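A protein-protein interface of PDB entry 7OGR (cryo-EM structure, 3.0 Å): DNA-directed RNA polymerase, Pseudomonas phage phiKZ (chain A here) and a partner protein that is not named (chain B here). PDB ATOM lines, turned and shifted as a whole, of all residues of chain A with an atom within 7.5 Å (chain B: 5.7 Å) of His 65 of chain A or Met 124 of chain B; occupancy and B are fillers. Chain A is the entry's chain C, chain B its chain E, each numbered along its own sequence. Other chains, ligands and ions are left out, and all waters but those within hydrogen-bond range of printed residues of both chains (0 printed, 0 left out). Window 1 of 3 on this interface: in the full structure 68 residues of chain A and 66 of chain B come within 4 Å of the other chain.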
ATOM      1  N   LYS A  62      -6.231   0.411  20.319  1.00  0.00           N
ATOM      2  CA  LYS A  62      -7.353  -0.035  19.508  1.00  0.00           C
ATOM      3  C   LYS A  62      -6.920  -0.805  18.268  1.00  0.00           C
ATOM      4  O   LYS A  62      -7.711  -1.595  17.740  1.00  0.00           O
ATOM      5  CB  LYS A  62      -8.205   1.170  19.085  1.00  0.00           C
ATOM      6  CG  LYS A  62      -9.645   0.841  18.724  1.00  0.00           C
ATOM      7  CD  LYS A  62     -10.277   1.957  17.911  1.00  0.00           C
ATOM      8  CE  LYS A  62     -10.561   3.175  18.769  1.00  0.00           C
ATOM      9  NZ  LYS A  62     -11.332   4.203  18.017  1.00  0.00           N
ATOM     10  N   TYR A  63      -5.686  -0.618  17.809  1.00  0.00           N
ATOM     11  CA  TYR A  63      -5.188  -1.244  16.586  1.00  0.00           C
ATOM     12  C   TYR A  63      -3.978  -2.098  16.951  1.00  0.00           C
ATOM     13  O   TYR A  63      -2.833  -1.649  16.861  1.00  0.00           O
ATOM     14  CB  TYR A  63      -4.839  -0.189  15.529  1.00  0.00           C
ATOM     15  CG  TYR A  63      -5.952   0.800  15.255  1.00  0.00           C
ATOM     16  CD1 TYR A  63      -6.952   0.512  14.333  1.00  0.00           C
ATOM     17  CD2 TYR A  63      -5.997   2.028  15.910  1.00  0.00           C
ATOM     18  CE1 TYR A  63      -7.972   1.413  14.078  1.00  0.00           C
ATOM     19  CE2 TYR A  63      -7.013   2.935  15.661  1.00  0.00           C
ATOM     20  CZ  TYR A  63      -7.996   2.621  14.744  1.00  0.00           C
ATOM     21  OH  TYR A  63      -9.006   3.520  14.493  1.00  0.00           O
ATOM     22  N   THR A  64      -4.241  -3.337  17.361  1.00  0.00           N
ATOM     23  CA  THR A  64      -3.205  -4.301  17.700  1.00  0.00           C
ATOM     24  C   THR A  64      -3.500  -5.618  16.999  1.00  0.00           C
ATOM     25  O   THR A  64      -4.632  -5.887  16.590  1.00  0.00           O
ATOM     26  CB  THR A  64      -3.109  -4.531  19.218  1.00  0.00           C
ATOM     27  OG1 THR A  64      -4.421  -4.728  19.759  1.00  0.00           O
ATOM     28  CG2 THR A  64      -2.454  -3.343  19.908  1.00  0.00           C
ATOM     29  N   HIS A  65      -2.463  -6.439  16.857  1.00  0.00           N
ATOM     30  CA  HIS A  65      -2.622  -7.753  16.245  1.00  0.00           C
ATOM     31  C   HIS A  65      -3.311  -8.698  17.222  1.00  0.00           C
ATOM     32  O   HIS A  65      -2.802  -8.947  18.320  1.00  0.00           O
ATOM     33  CB  HIS A  65      -1.267  -8.314  15.827  1.00  0.00           C
ATOM     34  CG  HIS A  65      -0.677  -7.645  14.625  1.00  0.00           C
ATOM     35  ND1 HIS A  65       0.393  -6.781  14.705  1.00  0.00           N
ATOM     36  CD2 HIS A  65      -1.009  -7.714  13.315  1.00  0.00           C
ATOM     37  CE1 HIS A  65       0.698  -6.349  13.493  1.00  0.00           C
ATOM     38  NE2 HIS A  65      -0.139  -6.899  12.633  1.00  0.00           N
ATOM     39  N   ASP A  66      -4.463  -9.227  16.824  1.00  0.00           N
ATOM     40  CA  ASP A  66      -5.229 -10.146  17.657  1.00  0.00           C
ATOM     41  C   ASP A  66      -6.098 -11.008  16.746  1.00  0.00           C
ATOM     42  O   ASP A  66      -5.916 -11.031  15.524  1.00  0.00           O
ATOM     43  CB  ASP A  66      -6.063  -9.384  18.694  1.00  0.00           C
ATOM     44  CG  ASP A  66      -6.747  -8.156  18.115  1.00  0.00           C
ATOM     45  OD1 ASP A  66      -6.713  -7.967  16.881  1.00  0.00           O
ATOM     46  OD2 ASP A  66      -7.323  -7.374  18.901  1.00  0.00           O
ATOM     47  N   VAL A  67      -7.045 -11.720  17.347  1.00  0.00           N
ATOM     48  CA  VAL A  67      -8.031 -12.508  16.618  1.00  0.00           C
ATOM     49  C   VAL A  67      -9.341 -11.733  16.627  1.00  0.00           C
ATOM     50  O   VAL A  67      -9.804 -11.295  17.686  1.00  0.00           O
ATOM     51  CB  VAL A  67      -8.200 -13.905  17.241  1.00  0.00           C
ATOM     52  CG1 VAL A  67      -9.220 -14.719  16.469  1.00  0.00           C
ATOM     53  CG2 VAL A  67      -6.861 -14.627  17.291  1.00  0.00           C
ATOM     54  N   ARG A  68      -9.935 -11.549  15.451  1.00  0.00           N
ATOM     55  CA  ARG A  68     -11.077 -10.657  15.328  1.00  0.00           C
ATOM     56  C   ARG A  68     -12.053 -11.214  14.303  1.00  0.00           C
ATOM     57  O   ARG A  68     -11.642 -11.713  13.252  1.00  0.00           O
ATOM     58  CB  ARG A  68     -10.620  -9.249  14.923  1.00  0.00           C
ATOM     59  CG  ARG A  68     -11.690  -8.174  15.007  1.00  0.00           C
ATOM     60  CD  ARG A  68     -11.119  -6.815  14.629  1.00  0.00           C
ATOM     61  NE  ARG A  68     -10.262  -6.264  15.675  1.00  0.00           N
ATOM     62  CZ  ARG A  68     -10.643  -5.330  16.538  1.00  0.00           C
ATOM     63  NH1 ARG A  68      -9.797  -4.888  17.458  1.00  0.00           N
ATOM     64  NH2 ARG A  68     -11.871  -4.834  16.484  1.00  0.00           N
ATOM     65  N   MET A 120       1.385 -15.205  19.322  1.00  0.00           N
ATOM     66  CA  MET A 120       1.686 -14.566  18.051  1.00  0.00           C
ATOM     67  C   MET A 120       3.101 -14.013  18.116  1.00  0.00           C
ATOM     68  O   MET A 120       3.517 -13.480  19.148  1.00  0.00           O
ATOM     69  CB  MET A 120       0.689 -13.447  17.723  1.00  0.00           C
ATOM     70  CG  MET A 120       0.335 -13.355  16.247  1.00  0.00           C
ATOM     71  SD  MET A 120      -0.986 -12.179  15.898  1.00  0.00           S
ATOM     72  CE  MET A 120      -2.334 -12.893  16.832  1.00  0.00           C
ATOM     73  N   SER A 121       3.835 -14.142  17.013  1.00  0.00           N
ATOM     74  CA  SER A 121       5.240 -13.742  16.988  1.00  0.00           C
ATOM     75  C   SER A 121       5.581 -13.259  15.586  1.00  0.00           C
ATOM     76  O   SER A 121       5.685 -14.066  14.659  1.00  0.00           O
ATOM     77  CB  SER A 121       6.145 -14.898  17.405  1.00  0.00           C
ATOM     78  OG  SER A 121       7.511 -14.526  17.343  1.00  0.00           O
ATOM     79  N   HIS A 122       5.758 -11.947  15.437  1.00  0.00           N
ATOM     80  CA  HIS A 122       6.175 -11.368  14.168  1.00  0.00           C
ATOM     81  C   HIS A 122       7.681 -11.172  14.081  1.00  0.00           C
ATOM     82  O   HIS A 122       8.205 -10.958  12.982  1.00  0.00           O
ATOM     83  CB  HIS A 122       5.474 -10.027  13.946  1.00  0.00           C
ATOM     84  CG  HIS A 122       4.119  -9.944  14.579  1.00  0.00           C
ATOM     85  ND1 HIS A 122       3.068 -10.748  14.195  1.00  0.00           N
ATOM     86  CD2 HIS A 122       3.646  -9.154  15.571  1.00  0.00           C
ATOM     87  CE1 HIS A 122       2.005 -10.456  14.923  1.00  0.00           C
ATOM     88  NE2 HIS A 122       2.329  -9.493  15.765  1.00  0.00           N
ATOM     89  N   TYR A 128       4.652 -12.860  21.968  1.00  0.00           N
ATOM     90  CA  TYR A 128       3.706 -12.628  23.051  1.00  0.00           C
ATOM     91  C   TYR A 128       2.557 -13.615  22.915  1.00  0.00           C
ATOM     92  O   TYR A 128       2.316 -14.173  21.842  1.00  0.00           O
ATOM     93  CB  TYR A 128       3.188 -11.182  23.056  1.00  0.00           C
ATOM     94  CG  TYR A 128       2.351 -10.786  21.854  1.00  0.00           C
ATOM     95  CD1 TYR A 128       2.949 -10.440  20.646  1.00  0.00           C
ATOM     96  CD2 TYR A 128       0.964 -10.741  21.936  1.00  0.00           C
ATOM     97  CE1 TYR A 128       2.187 -10.076  19.550  1.00  0.00           C
ATOM     98  CE2 TYR A 128       0.194 -10.378  20.846  1.00  0.00           C
ATOM     99  CZ  TYR A 128       0.812 -10.046  19.657  1.00  0.00           C
ATOM    100  OH  TYR A 128       0.050  -9.683  18.573  1.00  0.00           O
ATOM    101  N   GLU A 129       1.848 -13.821  24.021  1.00  0.00           N
ATOM    102  CA  GLU A 129       0.740 -14.762  24.080  1.00  0.00           C
ATOM    103  C   GLU A 129      -0.590 -14.044  23.866  1.00  0.00           C
ATOM    104  O   GLU A 129      -0.672 -12.814  23.857  1.00  0.00           O
ATOM    105  CB  GLU A 129       0.733 -15.504  25.419  1.00  0.00           C
ATOM    106  CG  GLU A 129       0.216 -14.680  26.584  1.00  0.00           C
ATOM    107  CD  GLU A 129       0.078 -15.494  27.854  1.00  0.00           C
ATOM    108  OE1 GLU A 129       0.413 -16.696  27.829  1.00  0.00           O
ATOM    109  OE2 GLU A 129      -0.363 -14.932  28.877  1.00  0.00           O
ATOM    110  N   LEU A 130      -1.643 -14.840  23.695  1.00  0.00           N
ATOM    111  CA  LEU A 130      -2.984 -14.339  23.404  1.00  0.00           C
ATOM    112  C   LEU A 130      -3.906 -14.699  24.567  1.00  0.00           C
ATOM    113  O   LEU A 130      -4.349 -15.845  24.686  1.00  0.00           O
ATOM    114  CB  LEU A 130      -3.501 -14.913  22.089  1.00  0.00           C
ATOM    115  CG  LEU A 130      -2.790 -14.460  20.813  1.00  0.00           C
ATOM    116  CD1 LEU A 130      -3.262 -15.277  19.623  1.00  0.00           C
ATOM    117  CD2 LEU A 130      -3.005 -12.975  20.573  1.00  0.00           C
ATOM    118  N   ALA A 153      -9.142 -13.515  22.238  1.00  0.00           N
ATOM    119  CA  ALA A 153      -7.687 -13.692  22.341  1.00  0.00           C
ATOM    120  C   ALA A 153      -6.936 -12.372  22.126  1.00  0.00           C
ATOM    121  O   ALA A 153      -6.202 -12.185  21.154  1.00  0.00           O
ATOM    122  CB  ALA A 153      -7.190 -14.782  21.381  1.00  0.00           C
ATOM    123  N   GLN A 154      -7.157 -11.450  23.060  1.00  0.00           N
ATOM    124  CA  GLN A 154      -6.388 -10.215  23.072  1.00  0.00           C
ATOM    125  C   GLN A 154      -4.977 -10.462  23.605  1.00  0.00           C
ATOM    126  O   GLN A 154      -4.652 -11.531  24.127  1.00  0.00           O
ATOM    127  CB  GLN A 154      -7.071  -9.149  23.929  1.00  0.00           C
ATOM    128  CG  GLN A 154      -7.967  -8.199  23.168  1.00  0.00           C
ATOM    129  CD  GLN A 154      -8.543  -7.112  24.052  1.00  0.00           C
ATOM    130  OE1 GLN A 154      -8.342  -7.114  25.266  1.00  0.00           O
ATOM    131  NE2 GLN A 154      -9.259  -6.172  23.446  1.00  0.00           N
ATOM    132  N   SER A 155      -4.138  -9.439  23.478  1.00  0.00           N
ATOM    133  CA  SER A 155      -2.802  -9.473  24.048  1.00  0.00           C
ATOM    134  C   SER A 155      -2.856  -9.085  25.524  1.00  0.00           C
ATOM    135  O   SER A 155      -3.915  -8.782  26.081  1.00  0.00           O
ATOM    136  CB  SER A 155      -1.868  -8.551  23.268  1.00  0.00           C
ATOM    137  OG  SER A 155      -0.571  -8.539  23.837  1.00  0.00           O
ATOM    138  N   VAL A 158      -3.063  -4.775  26.340  1.00  0.00           N
ATOM    139  CA  VAL A 158      -4.349  -4.088  26.284  1.00  0.00           C
ATOM    140  C   VAL A 158      -5.124  -4.429  27.552  1.00  0.00           C
ATOM    141  O   VAL A 158      -5.480  -5.588  27.782  1.00  0.00           O
ATOM    142  CB  VAL A 158      -5.140  -4.479  25.032  1.00  0.00           C
ATOM    143  CG1 VAL A 158      -6.487  -3.772  25.015  1.00  0.00           C
ATOM    144  CG2 VAL A 158      -4.342  -4.158  23.779  1.00  0.00           C
ATOM    145  N   ASP B  94       0.111 -16.936   1.655  1.00  0.00           N
ATOM    146  CA  ASP B  94      -1.247 -16.490   1.371  1.00  0.00           C
ATOM    147  C   ASP B  94      -1.402 -16.353  -0.138  1.00  0.00           C
ATOM    148  O   ASP B  94      -0.850 -15.429  -0.742  1.00  0.00           O
ATOM    149  CB  ASP B  94      -1.539 -15.169   2.078  1.00  0.00           C
ATOM    150  CG  ASP B  94      -1.553 -15.306   3.586  1.00  0.00           C
ATOM    151  OD1 ASP B  94      -1.878 -16.405   4.081  1.00  0.00           O
ATOM    152  OD2 ASP B  94      -1.241 -14.314   4.277  1.00  0.00           O
ATOM    153  N   PHE B 119      -3.575 -10.235   0.782  1.00  0.00           N
ATOM    154  CA  PHE B 119      -3.166  -9.484   1.964  1.00  0.00           C
ATOM    155  C   PHE B 119      -4.104  -9.744   3.146  1.00  0.00           C
ATOM    156  O   PHE B 119      -5.198 -10.299   3.008  1.00  0.00           O
ATOM    157  CB  PHE B 119      -3.119  -7.988   1.656  1.00  0.00           C
ATOM    158  CG  PHE B 119      -1.824  -7.537   1.048  1.00  0.00           C
ATOM    159  CD1 PHE B 119      -1.523  -7.829  -0.273  1.00  0.00           C
ATOM    160  CD2 PHE B 119      -0.908  -6.816   1.799  1.00  0.00           C
ATOM    161  CE1 PHE B 119      -0.329  -7.417  -0.833  1.00  0.00           C
ATOM    162  CE2 PHE B 119       0.288  -6.398   1.244  1.00  0.00           C
ATOM    163  CZ  PHE B 119       0.577  -6.698  -0.075  1.00  0.00           C
ATOM    164  N   LYS B 120      -3.657  -9.331   4.329  1.00  0.00           N
ATOM    165  CA  LYS B 120      -4.396  -9.489   5.576  1.00  0.00           C
ATOM    166  C   LYS B 120      -4.589  -8.129   6.245  1.00  0.00           C
ATOM    167  O   LYS B 120      -4.206  -7.086   5.710  1.00  0.00           O
ATOM    168  CB  LYS B 120      -3.680 -10.458   6.521  1.00  0.00           C
ATOM    169  CG  LYS B 120      -3.441 -11.843   5.945  1.00  0.00           C
ATOM    170  CD  LYS B 120      -4.747 -12.602   5.779  1.00  0.00           C
ATOM    171  CE  LYS B 120      -4.545 -13.879   4.982  1.00  0.00           C
ATOM    172  NZ  LYS B 120      -5.786 -14.297   4.277  1.00  0.00           N
ATOM    173  N   ARG B 121      -5.191  -8.154   7.434  1.00  0.00           N
ATOM    174  CA  ARG B 121      -5.450  -6.929   8.179  1.00  0.00           C
ATOM    175  C   ARG B 121      -4.158  -6.389   8.783  1.00  0.00           C
ATOM    176  O   ARG B 121      -3.435  -7.111   9.475  1.00  0.00           O
ATOM    177  CB  ARG B 121      -6.478  -7.182   9.281  1.00  0.00           C
ATOM    178  CG  ARG B 121      -6.517  -6.099  10.351  1.00  0.00           C
ATOM    179  CD  ARG B 121      -7.607  -6.343  11.377  1.00  0.00           C
ATOM    180  NE  ARG B 121      -7.778  -5.192  12.259  1.00  0.00           N
ATOM    181  CZ  ARG B 121      -7.406  -5.164  13.534  1.00  0.00           C
ATOM    182  NH1 ARG B 121      -7.600  -4.073  14.261  1.00  0.00           N
ATOM    183  NH2 ARG B 121      -6.835  -6.228  14.083  1.00  0.00           N
ATOM    184  N   GLY B 122      -3.872  -5.121   8.519  1.00  0.00           N
ATOM    185  CA  GLY B 122      -2.688  -4.480   9.043  1.00  0.00           C
ATOM    186  C   GLY B 122      -1.486  -4.507   8.132  1.00  0.00           C
ATOM    187  O   GLY B 122      -0.365  -4.335   8.628  1.00  0.00           O
ATOM    188  N   ASN B 123      -1.692  -4.708   6.824  1.00  0.00           N
ATOM    189  CA  ASN B 123      -0.643  -4.870   5.809  1.00  0.00           C
ATOM    190  C   ASN B 123       0.306  -6.009   6.191  1.00  0.00           C
ATOM    191  O   ASN B 123       1.508  -5.824   6.376  1.00  0.00           O
ATOM    192  CB  ASN B 123       0.122  -3.559   5.567  1.00  0.00           C
ATOM    193  CG  ASN B 123      -0.796  -2.376   5.288  1.00  0.00           C
ATOM    194  OD1 ASN B 123      -0.471  -1.238   5.625  1.00  0.00           O
ATOM    195  ND2 ASN B 123      -1.937  -2.637   4.663  1.00  0.00           N
ATOM    196  N   MET B 124      -0.269  -7.203   6.307  1.00  0.00           N
ATOM    197  CA  MET B 124       0.388  -8.357   6.914  1.00  0.00           C
ATOM    198  C   MET B 124       0.371  -9.541   5.950  1.00  0.00           C
ATOM    199  O   MET B 124      -0.083 -10.642   6.273  1.00  0.00           O
ATOM    200  CB  MET B 124      -0.270  -8.703   8.248  1.00  0.00           C
ATOM    201  CG  MET B 124       0.605  -9.506   9.207  1.00  0.00           C
ATOM    202  SD  MET B 124      -0.261  -9.958  10.719  1.00  0.00           S
ATOM    203  CE  MET B 124       0.953 -11.018  11.495  1.00  0.00           C
ATOM    204  N   VAL B 125       0.818  -9.304   4.716  1.00  0.00           N
ATOM    205  CA  VAL B 125       0.943 -10.385   3.748  1.00  0.00           C
ATOM    206  C   VAL B 125       2.072 -11.328   4.168  1.00  0.00           C
ATOM    207  O   VAL B 125       3.016 -10.939   4.872  1.00  0.00           O
ATOM    208  CB  VAL B 125       1.153  -9.806   2.331  1.00  0.00           C
ATOM    209  CG1 VAL B 125       2.577  -9.306   2.116  1.00  0.00           C
ATOM    210  CG2 VAL B 125       0.752 -10.804   1.254  1.00  0.00           C
ATOM    211  N   THR B 126       1.939 -12.599   3.793  1.00  0.00           N
ATOM    212  CA  THR B 126       2.918 -13.629   4.118  1.00  0.00           C
ATOM    213  C   THR B 126       3.233 -14.409   2.851  1.00  0.00           C
ATOM    214  O   THR B 126       2.338 -15.027   2.264  1.00  0.00           O
ATOM    215  CB  THR B 126       2.397 -14.566   5.211  1.00  0.00           C
ATOM    216  OG1 THR B 126       2.144 -13.816   6.405  1.00  0.00           O
ATOM    217  CG2 THR B 126       3.417 -15.650   5.512  1.00  0.00           C
ATOM    218  N   LYS B 131       6.978 -13.284   6.718  1.00  0.00           N
ATOM    219  CA  LYS B 131       5.988 -12.218   6.756  1.00  0.00           C
ATOM    220  C   LYS B 131       6.531 -10.965   6.084  1.00  0.00           C
ATOM    221  O   LYS B 131       7.719 -10.647   6.196  1.00  0.00           O
ATOM    222  CB  LYS B 131       5.597 -11.906   8.201  1.00  0.00           C
ATOM    223  CG  LYS B 131       5.102 -13.109   8.983  1.00  0.00           C
ATOM    224  CD  LYS B 131       4.437 -12.684  10.281  1.00  0.00           C
ATOM    225  CE  LYS B 131       3.999 -13.889  11.095  1.00  0.00           C
ATOM    226  NZ  LYS B 131       3.255 -13.486  12.320  1.00  0.00           N
ATOM    227  N   TYR B 132       5.655 -10.252   5.383  1.00  0.00           N
ATOM    228  CA  TYR B 132       6.021  -9.025   4.693  1.00  0.00           C
ATOM    229  C   TYR B 132       4.990  -7.945   4.992  1.00  0.00           C
ATOM    230  O   TYR B 132       3.967  -8.189   5.637  1.00  0.00           O
ATOM    231  CB  TYR B 132       6.147  -9.248   3.180  1.00  0.00           C
ATOM    232  CG  TYR B 132       7.383 -10.018   2.775  1.00  0.00           C
ATOM    233  CD1 TYR B 132       7.378 -11.408   2.737  1.00  0.00           C
ATOM    234  CD2 TYR B 132       8.556  -9.356   2.433  1.00  0.00           C
ATOM    235  CE1 TYR B 132       8.507 -12.117   2.367  1.00  0.00           C
ATOM    236  CE2 TYR B 132       9.691 -10.055   2.062  1.00  0.00           C
ATOM    237  CZ  TYR B 132       9.659 -11.435   2.033  1.00  0.00           C
ATOM    238  OH  TYR B 132      10.784 -12.137   1.665  1.00  0.00           O
ATOM    239  N   ILE B 133       5.272  -6.735   4.514  1.00  0.00           N
ATOM    240  CA  ILE B 133       4.433  -5.568   4.766  1.00  0.00           C
ATOM    241  C   ILE B 133       4.300  -4.784   3.466  1.00  0.00           C
ATOM    242  O   ILE B 133       5.307  -4.416   2.853  1.00  0.00           O
ATOM    243  CB  ILE B 133       5.010  -4.682   5.892  1.00  0.00           C
ATOM    244  CG1 ILE B 133       4.663  -5.260   7.265  1.00  0.00           C
ATOM    245  CG2 ILE B 133       4.497  -3.250   5.802  1.00  0.00           C
ATOM    246  CD1 ILE B 133       5.388  -4.587   8.407  1.00  0.00           C
ATOM    247  N   GLY B 134       3.062  -4.544   3.040  1.00  0.00           N
ATOM    248  CA  GLY B 134       2.806  -3.710   1.878  1.00  0.00           C
ATOM    249  C   GLY B 134       2.627  -2.255   2.280  1.00  0.00           C
ATOM    250  O   GLY B 134       1.940  -1.943   3.251  1.00  0.00           O
ATOM    251  N   MET B 448       8.736  -7.888   7.717  1.00  0.00           N
ATOM    252  CA  MET B 448       8.119  -7.566   8.999  1.00  0.00           C
ATOM    253  C   MET B 448       9.009  -8.054  10.136  1.00  0.00           C
ATOM    254  O   MET B 448       9.308  -9.250  10.229  1.00  0.00           O
ATOM    255  CB  MET B 448       6.732  -8.194   9.094  1.00  0.00           C
ATOM    256  CG  MET B 448       5.943  -7.766  10.319  1.00  0.00           C
ATOM    257  SD  MET B 448       4.450  -8.742  10.565  1.00  0.00           S
ATOM    258  CE  MET B 448       3.544  -7.685  11.690  1.00  0.00           C
ATOM    259  N   ASN B 450       8.514  -6.866  13.655  1.00  0.00           N
ATOM    260  CA  ASN B 450       7.902  -6.186  14.790  1.00  0.00           C
ATOM    261  C   ASN B 450       7.938  -7.077  16.024  1.00  0.00           C
ATOM    262  O   ASN B 450       7.349  -8.166  16.005  1.00  0.00           O
ATOM    263  CB  ASN B 450       6.464  -5.809  14.471  1.00  0.00           C
ATOM    264  CG  ASN B 450       5.821  -4.987  15.570  1.00  0.00           C
ATOM    265  OD1 ASN B 450       6.483  -4.190  16.234  1.00  0.00           O
ATOM    266  ND2 ASN B 450       4.523  -5.181  15.770  1.00  0.00           N
ATOM    267  N   ASN B 452       6.478  -6.240  18.870  1.00  0.00           N
ATOM    268  CA  ASN B 452       5.431  -5.714  19.732  1.00  0.00           C
ATOM    269  C   ASN B 452       4.069  -6.102  19.171  1.00  0.00           C
ATOM    270  O   ASN B 452       3.949  -6.588  18.043  1.00  0.00           O
ATOM    271  CB  ASN B 452       5.542  -4.188  19.868  1.00  0.00           C
ATOM    272  CG  ASN B 452       5.074  -3.689  21.217  1.00  0.00           C
ATOM    273  OD1 ASN B 452       4.766  -4.476  22.111  1.00  0.00           O
ATOM    274  ND2 ASN B 452       5.013  -2.371  21.372  1.00  0.00           N
ATOM    275  N   SER B 453       3.032  -5.877  19.980  1.00  0.00           N
ATOM    276  CA  SER B 453       1.675  -6.230  19.581  1.00  0.00           C
ATOM    277  C   SER B 453       1.047  -5.184  18.668  1.00  0.00           C
ATOM    278  O   SER B 453       0.193  -5.527  17.842  1.00  0.00           O
ATOM    279  CB  SER B 453       0.803  -6.431  20.821  1.00  0.00           C
ATOM    280  OG  SER B 453      -0.513  -6.817  20.464  1.00  0.00           O
ATOM    281  N   SER B 454       1.444  -3.922  18.805  1.00  0.00           N
ATOM    282  CA  SER B 454       0.835  -2.844  18.038  1.00  0.00           C
ATOM    283  C   SER B 454       1.270  -2.888  16.577  1.00  0.00           C
ATOM    284  O   SER B 454       2.363  -3.352  16.241  1.00  0.00           O
ATOM    285  CB  SER B 454       1.196  -1.489  18.647  1.00  0.00           C
ATOM    286  OG  SER B 454       0.560  -0.430  17.954  1.00  0.00           O
ATOM    287  N   MET B 455       0.391  -2.397  15.702  1.00  0.00           N
ATOM    288  CA  MET B 455       0.669  -2.312  14.277  1.00  0.00           C
ATOM    289  C   MET B 455       0.834  -0.885  13.775  1.00  0.00           C
ATOM    290  O   MET B 455       1.185  -0.696  12.606  1.00  0.00           O
ATOM    291  CB  MET B 455      -0.449  -2.995  13.475  1.00  0.00           C
ATOM    292  CG  MET B 455      -1.835  -2.435  13.747  1.00  0.00           C
ATOM    293  SD  MET B 455      -3.117  -3.204  12.739  1.00  0.00           S
ATOM    294  CE  MET B 455      -3.195  -4.834  13.473  1.00  0.00           C
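A ring nitrogen (NE2) of His 122 of chain A is in hydrogen-bond range of a ring nitrogen (ND1) of His 65 of chain A, at 3.5 Å. OH of Tyr 128 of chain A lies within hydrogen-bond range of O of His 65 of chain A (3.0 Å). The guanidinium group (NH1) of Arg 68 of chain A is in salt-bridge range of the side-chain carboxylate (OD2) of Asp 66 of chain A (3.8 Å). The backbone NH (N) of Met 448 of chain B lies within hydrogen-bond range of the backbone carbonyl oxygen (O) of Lys 131 of chain B, at 3.3 Å. The side-chain amide nitrogen (ND2) of Asn 450 of chain B sits at hydrogen-bond distance from the backbone carbonyl oxygen (O) of Asn 452 of chain B, at 2.7 Å. The side-chain amide nitrogen (ND2) of Asn 450 of chain B is in hydrogen-bond range of the backbone carbonyl oxygen (O) of Ser 454 of chain B, at 2.9 Å.
The guanidinium group (NH2) of Arg 121 of chain B sits at hydrogen-bond distance from the backbone carbonyl oxygen (O) of Thr 64 of chain A, 3.4 Å away. The side-chain sulfur of Met 124 of chain B lies close to a ring nitrogen (NE2) of His 65 of chain A. The backbone carbonyl oxygen of Ser 453 of chain B is in hydrogen-bond range of the backbone NH of His 65 of chain A (3.0 Å). The guanidinium group (NH2) of Arg 121 of chain B is in salt-bridge range of the side-chain carboxylate (OD1) of Asp 66 of chain A, at 3.3 Å. The backbone carbonyl oxygen of Ser 121 of chain A is in hydrogen-bond range of the side-chain amino group of Lys 131 of chain B (3.4 Å). ND1 of His 122 of chain A is in hydrogen-bond range of NZ of Lys 131 of chain B (3.3 Å). The side-chain hydroxyl of Tyr 128 of chain A lies within hydrogen-bond range of the side-chain hydroxyl of Ser 453 of chain B, at 3.5 Å. The backbone carbonyl oxygen of Met 448 of chain B sits close to the backbone carbonyl oxygen of His 122 of chain A (3.4 Å).
His 65 of chain A touches just these residues of chain B: Met 124 (3.5 Å), Met 448 (3.6 Å), Ser 453 (3.0 Å) and Met 455 (3.5 Å). Met 124 of chain B touches two residues of chain A. Printed residues of chain A within 4 Å of Ser 454 of chain B: Tyr 63 (3.8 Å) and Thr 64 (3.8 Å). Of the printed residues of chain A, Met 455 of chain B touches Tyr 63, Thr 64 and His 65. Asn 123 of chain B touches none of the printed residues of chain A. Lys 62 of chain A touches none of the printed residues of chain B. The nearest residue of chain A that does not touch Met 124 of chain B is Met 120 of chain A (4.9 Å). The nearest printed residue of chain B that does not touch Arg 68 of chain A is Met 455 of chain B (7.5 Å).
O of Tyr 63 of chain A touches OG of Ser 454 of chain B, at 3.8 Å. Tyr 63 of chain A touches Met 455 of chain B (O to CG, 3.4 Å). Thr 64 of chain A touches Ser 454 of chain B. Met 455 of chain B touches Thr 64 of chain A (CE to O, 3.6 Å). His 65 of chain A touches Met 448 of chain B. His 65 of chain A touches Met 455 of chain B (CE1 to CB, 3.5 Å). NE of Arg 68 of chain A touches NH1 of Arg 121 of chain B, 3.7 Å away. Asn 450 of chain B touches His 122 of chain A (O to CB, 3.3 Å). His 122 of chain A touches Asn 452 of chain B (CD2 to O, 3.6 Å). Ser 155 of chain A touches Ser 453 of chain B.
Of the 19 printed residues of chain B, 9 touch a printed residue of chain A. Hydrophobic or aromatic side chains of chain B within 4 Å of the printed part of chain A: Met 124, Met 448 and Met 455. Hydrophobic or aromatic side chains of chain A within 4 Å of the printed part of chain B: His 65, His 122 and Tyr 128. Among the printed residues, 20 pairs touch across the chains. Among the printed residues, Asp or Glu carboxylates within 4 Å of a Lys or Arg side-chain nitrogen of the other chain: Asp 66 of chain A with Arg 121 of chain B.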
